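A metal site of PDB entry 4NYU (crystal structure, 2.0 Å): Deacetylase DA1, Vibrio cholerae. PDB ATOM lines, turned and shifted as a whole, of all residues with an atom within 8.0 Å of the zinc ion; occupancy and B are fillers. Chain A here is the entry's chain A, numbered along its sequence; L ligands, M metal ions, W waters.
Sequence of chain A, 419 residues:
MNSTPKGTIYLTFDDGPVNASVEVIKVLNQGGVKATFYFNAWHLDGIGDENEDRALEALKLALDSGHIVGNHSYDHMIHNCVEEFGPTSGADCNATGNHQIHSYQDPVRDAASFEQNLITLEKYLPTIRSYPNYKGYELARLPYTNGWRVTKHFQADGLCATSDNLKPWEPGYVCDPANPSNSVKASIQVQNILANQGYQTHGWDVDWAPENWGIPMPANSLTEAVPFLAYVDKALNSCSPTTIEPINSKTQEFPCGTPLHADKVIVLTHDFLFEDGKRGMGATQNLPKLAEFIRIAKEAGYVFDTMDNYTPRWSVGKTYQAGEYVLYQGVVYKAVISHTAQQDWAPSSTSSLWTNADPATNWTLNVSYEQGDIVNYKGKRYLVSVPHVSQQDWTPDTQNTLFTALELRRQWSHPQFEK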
ATOM      1  N   PHE A  13      23.704   2.031  14.450  1.00  0.00           N
ATOM      2  CA  PHE A  13      23.500   2.029  13.004  1.00  0.00           C
ATOM      3  C   PHE A  13      24.832   2.102  12.271  1.00  0.00           C
ATOM      4  O   PHE A  13      25.639   2.993  12.537  1.00  0.00           O
ATOM      5  CB  PHE A  13      22.621   3.221  12.602  1.00  0.00           C
ATOM      6  CG  PHE A  13      21.228   3.162  13.168  1.00  0.00           C
ATOM      7  CD1 PHE A  13      20.172   2.695  12.391  1.00  0.00           C
ATOM      8  CD2 PHE A  13      20.970   3.578  14.458  1.00  0.00           C
ATOM      9  CE1 PHE A  13      18.895   2.644  12.907  1.00  0.00           C
ATOM     10  CE2 PHE A  13      19.692   3.528  14.983  1.00  0.00           C
ATOM     11  CZ  PHE A  13      18.646   3.067  14.206  1.00  0.00           C
ATOM     12  N   ASP A  14      25.053   1.180  11.342  1.00  0.00           N
ATOM     13  CA  ASP A  14      26.330   1.078  10.645  1.00  0.00           C
ATOM     14  C   ASP A  14      26.239   1.528   9.191  1.00  0.00           C
ATOM     15  O   ASP A  14      25.174   1.455   8.570  1.00  0.00           O
ATOM     16  CB  ASP A  14      26.856  -0.355  10.709  1.00  0.00           C
ATOM     17  CG  ASP A  14      27.436  -0.708  12.059  1.00  0.00           C
ATOM     18  OD1 ASP A  14      27.238   0.065  13.019  1.00  0.00           O
ATOM     19  OD2 ASP A  14      28.099  -1.763  12.162  1.00  0.00           O
ATOM     20  N   ASP A  15      27.368   1.996   8.667  1.00  0.00           N
ATOM     21  CA  ASP A  15      27.565   2.239   7.231  1.00  0.00           C
ATOM     22  C   ASP A  15      27.068   3.602   6.720  1.00  0.00           C
ATOM     23  O   ASP A  15      27.177   3.890   5.535  1.00  0.00           O
ATOM     24  CB  ASP A  15      26.976   1.108   6.385  1.00  0.00           C
ATOM     25  CG  ASP A  15      27.681  -0.227   6.619  1.00  0.00           C
ATOM     26  OD1 ASP A  15      28.305  -0.406   7.691  1.00  0.00           O
ATOM     27  OD2 ASP A  15      27.595  -1.101   5.731  1.00  0.00           O
ATOM     28  N   GLY A  16      26.527   4.434   7.607  1.00  0.00           N
ATOM     29  CA  GLY A  16      26.176   5.800   7.240  1.00  0.00           C
ATOM     30  C   GLY A  16      27.445   6.630   7.108  1.00  0.00           C
ATOM     31  O   GLY A  16      28.538   6.090   7.227  1.00  0.00           O
ATOM     32  N   TYR A  38      27.917   4.332  13.588  1.00  0.00           N
ATOM     33  CA  TYR A  38      29.269   4.001  13.163  1.00  0.00           C
ATOM     34  C   TYR A  38      29.415   4.289  11.680  1.00  0.00           C
ATOM     35  O   TYR A  38      28.940   3.517  10.841  1.00  0.00           O
ATOM     36  CB  TYR A  38      29.589   2.538  13.483  1.00  0.00           C
ATOM     37  CG  TYR A  38      29.690   2.253  14.968  1.00  0.00           C
ATOM     38  CD1 TYR A  38      30.878   2.484  15.660  1.00  0.00           C
ATOM     39  CD2 TYR A  38      28.601   1.785  15.686  1.00  0.00           C
ATOM     40  CE1 TYR A  38      30.979   2.244  17.022  1.00  0.00           C
ATOM     41  CE2 TYR A  38      28.700   1.532  17.048  1.00  0.00           C
ATOM     42  CZ  TYR A  38      29.884   1.769  17.710  1.00  0.00           C
ATOM     43  OH  TYR A  38      29.992   1.521  19.062  1.00  0.00           O
ATOM     44  N   PHE A  39      30.054   5.409  11.354  1.00  0.00           N
ATOM     45  CA  PHE A  39      30.054   5.953  10.003  1.00  0.00           C
ATOM     46  C   PHE A  39      31.280   5.588   9.167  1.00  0.00           C
ATOM     47  O   PHE A  39      32.378   5.361   9.689  1.00  0.00           O
ATOM     48  CB  PHE A  39      29.964   7.475  10.051  1.00  0.00           C
ATOM     49  CG  PHE A  39      28.580   8.017  10.309  1.00  0.00           C
ATOM     50  CD1 PHE A  39      27.452   7.276  10.026  1.00  0.00           C
ATOM     51  CD2 PHE A  39      28.422   9.298  10.809  1.00  0.00           C
ATOM     52  CE1 PHE A  39      26.188   7.797  10.265  1.00  0.00           C
ATOM     53  CE2 PHE A  39      27.167   9.825  11.049  1.00  0.00           C
ATOM     54  CZ  PHE A  39      26.049   9.068  10.778  1.00  0.00           C
ATOM     55  N   ASN A  40      31.076   5.541   7.844  1.00  0.00           N
ATOM     56  CA  ASN A  40      32.157   5.485   6.876  1.00  0.00           C
ATOM     57  C   ASN A  40      32.169   6.782   6.082  1.00  0.00           C
ATOM     58  O   ASN A  40      31.196   7.105   5.394  1.00  0.00           O
ATOM     59  CB  ASN A  40      31.958   4.313   5.895  1.00  0.00           C
ATOM     60  CG  ASN A  40      31.724   2.996   6.611  1.00  0.00           C
ATOM     61  OD1 ASN A  40      30.668   2.374   6.447  1.00  0.00           O
ATOM     62  ND2 ASN A  40      32.705   2.544   7.378  1.00  0.00           N
ATOM     63  N   HIS A  72      33.771   3.594  11.841  1.00  0.00           N
ATOM     64  CA  HIS A  72      33.579   2.316  11.139  1.00  0.00           C
ATOM     65  C   HIS A  72      34.583   2.190   9.987  1.00  0.00           C
ATOM     66  O   HIS A  72      34.403   1.351   9.108  1.00  0.00           O
ATOM     67  CB  HIS A  72      32.134   2.251  10.615  1.00  0.00           C
ATOM     68  CG  HIS A  72      31.643   0.874  10.286  1.00  0.00           C
ATOM     69  ND1 HIS A  72      31.922  -0.227  11.072  1.00  0.00           N
ATOM     70  CD2 HIS A  72      30.862   0.423   9.280  1.00  0.00           C
ATOM     71  CE1 HIS A  72      31.350  -1.297  10.546  1.00  0.00           C
ATOM     72  NE2 HIS A  72      30.688  -0.929   9.469  1.00  0.00           N
ATOM     73  N   SER A  73      35.614   3.028  10.005  1.00  0.00           N
ATOM     74  CA  SER A  73      36.627   3.085   8.943  1.00  0.00           C
ATOM     75  C   SER A  73      36.162   3.949   7.763  1.00  0.00           C
ATOM     76  O   SER A  73      34.970   4.153   7.556  1.00  0.00           O
ATOM     77  CB  SER A  73      37.036   1.691   8.452  1.00  0.00           C
ATOM     78  OG  SER A  73      36.145   1.186   7.470  1.00  0.00           O
ATOM     79  N   HIS A  76      35.010   1.141   4.639  1.00  0.00           N
ATOM     80  CA  HIS A  76      34.464  -0.180   4.985  1.00  0.00           C
ATOM     81  C   HIS A  76      35.332  -1.302   4.416  1.00  0.00           C
ATOM     82  O   HIS A  76      34.836  -2.374   4.077  1.00  0.00           O
ATOM     83  CB  HIS A  76      33.034  -0.307   4.466  1.00  0.00           C
ATOM     84  CG  HIS A  76      32.176  -1.250   5.254  1.00  0.00           C
ATOM     85  ND1 HIS A  76      32.255  -2.621   5.135  1.00  0.00           N
ATOM     86  CD2 HIS A  76      31.218  -1.013   6.182  1.00  0.00           C
ATOM     87  CE1 HIS A  76      31.381  -3.190   5.949  1.00  0.00           C
ATOM     88  NE2 HIS A  76      30.737  -2.237   6.598  1.00  0.00           N
ATOM     89  N   ARG A 141      34.002   0.249  15.488  1.00  0.00           N
ATOM     90  CA  ARG A 141      33.511  -1.096  15.227  1.00  0.00           C
ATOM     91  C   ARG A 141      34.054  -1.563  13.885  1.00  0.00           C
ATOM     92  O   ARG A 141      34.002  -0.819  12.899  1.00  0.00           O
ATOM     93  CB  ARG A 141      31.985  -1.128  15.227  1.00  0.00           C
ATOM     94  CG  ARG A 141      31.396  -2.458  14.816  1.00  0.00           C
ATOM     95  CD  ARG A 141      29.886  -2.402  14.771  1.00  0.00           C
ATOM     96  NE  ARG A 141      29.289  -2.495  16.103  1.00  0.00           N
ATOM     97  CZ  ARG A 141      28.019  -2.188  16.375  1.00  0.00           C
ATOM     98  NH1 ARG A 141      27.206  -1.760  15.413  1.00  0.00           N
ATOM     99  NH2 ARG A 141      27.558  -2.302  17.609  1.00  0.00           N
ATOM    100  N   LEU A 142      34.588  -2.778  13.836  1.00  0.00           N
ATOM    101  CA  LEU A 142      35.197  -3.283  12.623  1.00  0.00           C
ATOM    102  C   LEU A 142      34.162  -3.822  11.631  1.00  0.00           C
ATOM    103  O   LEU A 142      33.265  -4.564  12.012  1.00  0.00           O
ATOM    104  CB  LEU A 142      36.195  -4.396  12.950  1.00  0.00           C
ATOM    105  CG  LEU A 142      37.661  -3.941  13.020  1.00  0.00           C
ATOM    106  CD1 LEU A 142      37.877  -3.053  14.230  1.00  0.00           C
ATOM    107  CD2 LEU A 142      38.583  -5.137  13.054  1.00  0.00           C
ATOM    108  N   PRO A 143      34.288  -3.426  10.361  1.00  0.00           N
ATOM    109  CA  PRO A 143      33.429  -3.956   9.303  1.00  0.00           C
ATOM    110  C   PRO A 143      33.381  -5.489   9.293  1.00  0.00           C
ATOM    111  O   PRO A 143      34.419  -6.132   9.444  1.00  0.00           O
ATOM    112  CB  PRO A 143      34.099  -3.441   8.022  1.00  0.00           C
ATOM    113  CG  PRO A 143      34.714  -2.153   8.438  1.00  0.00           C
ATOM    114  CD  PRO A 143      35.188  -2.364   9.850  1.00  0.00           C
ATOM    115  N   TYR A 144      32.187  -6.044   9.133  1.00  0.00           N
ATOM    116  CA  TYR A 144      32.007  -7.490   8.966  1.00  0.00           C
ATOM    117  C   TYR A 144      32.213  -8.293  10.241  1.00  0.00           C
ATOM    118  O   TYR A 144      31.928  -9.497  10.271  1.00  0.00           O
ATOM    119  CB  TYR A 144      32.950  -8.027   7.895  1.00  0.00           C
ATOM    120  CG  TYR A 144      33.030  -7.208   6.624  1.00  0.00           C
ATOM    121  CD1 TYR A 144      31.913  -7.039   5.812  1.00  0.00           C
ATOM    122  CD2 TYR A 144      34.231  -6.620   6.219  1.00  0.00           C
ATOM    123  CE1 TYR A 144      31.989  -6.294   4.636  1.00  0.00           C
ATOM    124  CE2 TYR A 144      34.305  -5.875   5.063  1.00  0.00           C
ATOM    125  CZ  TYR A 144      33.191  -5.713   4.272  1.00  0.00           C
ATOM    126  OH  TYR A 144      33.265  -4.967   3.116  1.00  0.00           O
ATOM    127  N   THR A 145      32.690  -7.649  11.298  1.00  0.00           N
ATOM    128  CA  THR A 145      33.290  -8.387  12.412  1.00  0.00           C
ATOM    129  C   THR A 145      32.644  -8.092  13.766  1.00  0.00           C
ATOM    130  O   THR A 145      32.639  -6.954  14.238  1.00  0.00           O
ATOM    131  CB  THR A 145      34.793  -8.084  12.504  1.00  0.00           C
ATOM    132  OG1 THR A 145      35.416  -8.349  11.237  1.00  0.00           O
ATOM    133  CG2 THR A 145      35.460  -8.939  13.581  1.00  0.00           C
ATOM    134  N   TRP A 204      27.936  -6.788  18.565  1.00  0.00           N
ATOM    135  CA  TRP A 204      26.498  -6.672  18.734  1.00  0.00           C
ATOM    136  C   TRP A 204      25.873  -7.961  19.272  1.00  0.00           C
ATOM    137  O   TRP A 204      26.464  -9.038  19.180  1.00  0.00           O
ATOM    138  CB  TRP A 204      25.824  -6.268  17.413  1.00  0.00           C
ATOM    139  CG  TRP A 204      26.082  -7.215  16.277  1.00  0.00           C
ATOM    140  CD1 TRP A 204      25.270  -8.234  15.868  1.00  0.00           C
ATOM    141  CD2 TRP A 204      27.210  -7.220  15.390  1.00  0.00           C
ATOM    142  NE1 TRP A 204      25.828  -8.875  14.790  1.00  0.00           N
ATOM    143  CE2 TRP A 204      27.015  -8.274  14.473  1.00  0.00           C
ATOM    144  CE3 TRP A 204      28.358  -6.427  15.290  1.00  0.00           C
ATOM    145  CZ2 TRP A 204      27.935  -8.557  13.465  1.00  0.00           C
ATOM    146  CZ3 TRP A 204      29.274  -6.723  14.292  1.00  0.00           C
ATOM    147  CH2 TRP A 204      29.056  -7.778  13.393  1.00  0.00           C
ATOM    148  N   LEU A 268      22.316  -4.136  16.261  1.00  0.00           N
ATOM    149  CA  LEU A 268      22.982  -3.713  15.036  1.00  0.00           C
ATOM    150  C   LEU A 268      21.974  -3.618  13.906  1.00  0.00           C
ATOM    151  O   LEU A 268      21.137  -4.506  13.737  1.00  0.00           O
ATOM    152  CB  LEU A 268      24.078  -4.704  14.649  1.00  0.00           C
ATOM    153  CG  LEU A 268      24.591  -4.582  13.208  1.00  0.00           C
ATOM    154  CD1 LEU A 268      25.409  -3.322  13.000  1.00  0.00           C
ATOM    155  CD2 LEU A 268      25.402  -5.814  12.822  1.00  0.00           C
ATOM    156  N   THR A 269      22.039  -2.535  13.140  1.00  0.00           N
ATOM    157  CA  THR A 269      21.277  -2.426  11.911  1.00  0.00           C
ATOM    158  C   THR A 269      21.975  -1.445  10.995  1.00  0.00           C
ATOM    159  O   THR A 269      23.030  -0.910  11.346  1.00  0.00           O
ATOM    160  CB  THR A 269      19.813  -1.982  12.178  1.00  0.00           C
ATOM    161  OG1 THR A 269      19.038  -2.152  10.985  1.00  0.00           O
ATOM    162  CG2 THR A 269      19.758  -0.524  12.616  1.00  0.00           C
ATOM    163  N   HIS A 270      21.403  -1.210   9.815  1.00  0.00           N
ATOM    164  CA  HIS A 270      22.032  -0.340   8.830  1.00  0.00           C
ATOM    165  C   HIS A 270      21.062   0.722   8.327  1.00  0.00           C
ATOM    166  O   HIS A 270      19.893   0.449   8.092  1.00  0.00           O
ATOM    167  CB  HIS A 270      22.563  -1.154   7.649  1.00  0.00           C
ATOM    168  CG  HIS A 270      23.582  -2.174   8.043  1.00  0.00           C
ATOM    169  ND1 HIS A 270      23.281  -3.277   8.809  1.00  0.00           N
ATOM    170  CD2 HIS A 270      24.906  -2.268   7.762  1.00  0.00           C
ATOM    171  CE1 HIS A 270      24.370  -4.003   8.989  1.00  0.00           C
ATOM    172  NE2 HIS A 270      25.367  -3.417   8.366  1.00  0.00           N
ATOM    173  N   PHE A 272      20.877   2.017   5.445  1.00  0.00           N
ATOM    174  CA  PHE A 272      20.403   1.780   4.081  1.00  0.00           C
ATOM    175  C   PHE A 272      19.202   0.840   4.014  1.00  0.00           C
ATOM    176  O   PHE A 272      18.565   0.704   2.972  1.00  0.00           O
ATOM    177  CB  PHE A 272      21.533   1.274   3.175  1.00  0.00           C
ATOM    178  CG  PHE A 272      22.175  -0.015   3.632  1.00  0.00           C
ATOM    179  CD1 PHE A 272      21.440  -1.191   3.702  1.00  0.00           C
ATOM    180  CD2 PHE A 272      23.515  -0.051   3.963  1.00  0.00           C
ATOM    181  CE1 PHE A 272      22.032  -2.362   4.108  1.00  0.00           C
ATOM    182  CE2 PHE A 272      24.112  -1.231   4.370  1.00  0.00           C
ATOM    183  CZ  PHE A 272      23.367  -2.390   4.437  1.00  0.00           C
HETATM  184  C1  LIG L   1      29.301  -3.909   9.896  1.00  0.00           C
HETATM  185  O1  LIG L   1      30.052  -3.929   8.896  1.00  0.00           O
HETATM  186  O2  LIG L   1      28.435  -3.008   9.895  1.00  0.00           O
HETATM  187  C2  LIG L   1      29.436  -4.884  11.014  1.00  0.00           C
HETATM  188 ZN    ZN M   1      29.422  -2.010   8.159  1.00  0.00          ZN
HETATM  189  O   HOH W   1      27.822  -3.683   6.877  1.00  0.00           O
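The backbone NH (N) of Asp 15 lies within hydrogen-bond range of the backbone carbonyl oxygen (O) of Tyr 38 (3.1 Å).
The side-chain hydroxyl (OH) of Tyr 144 sits at hydrogen-bond distance from the backbone carbonyl oxygen (O) of His 76 (3.2 Å).
N of His 76 lies within hydrogen-bond range of OG of Ser 73 (3.1 Å).
O of His 72 is in hydrogen-bond range of ND2 of Asn 40 (2.7 Å).
The backbone carbonyl oxygen (O) of Arg 141 lies within hydrogen-bond range of a ring nitrogen (ND1) of His 72, 2.8 Å away.
The backbone NH (N) of His 72 lies within hydrogen-bond range of the backbone carbonyl oxygen (O) of Phe 39, 3.1 Å away.
The side-chain carboxylate of Asp 14 is in salt-bridge range of the guanidinium group of Arg 141, at 3.0 Å.
N of Asp 14 is in hydrogen-bond range of O of Thr 269 (2.9 Å).
CB of Asp 14 touches the zinc ion, at 3.98 Å.
Four residues have an atom within 4 Å of the zinc ion: Asp 14, Asp 15, His 72 and His 76.
The zinc ion is bound by OD1 of Asp 15 (2.0 Å), NE2 of His 76 (2.1 Å), NE2 of His 72 (2.1 Å), O1 of the ligand (2.2 Å) and O2 of the ligand (2.2 Å).
The zinc ion has five donor atoms within binding distance.
Slightly farther from the zinc ion lies water W1 (2.6 Å).
Water W1 bridges OD2 of Asp 15 (2.8 Å) and NE2 of His 270 (2.9 Å).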
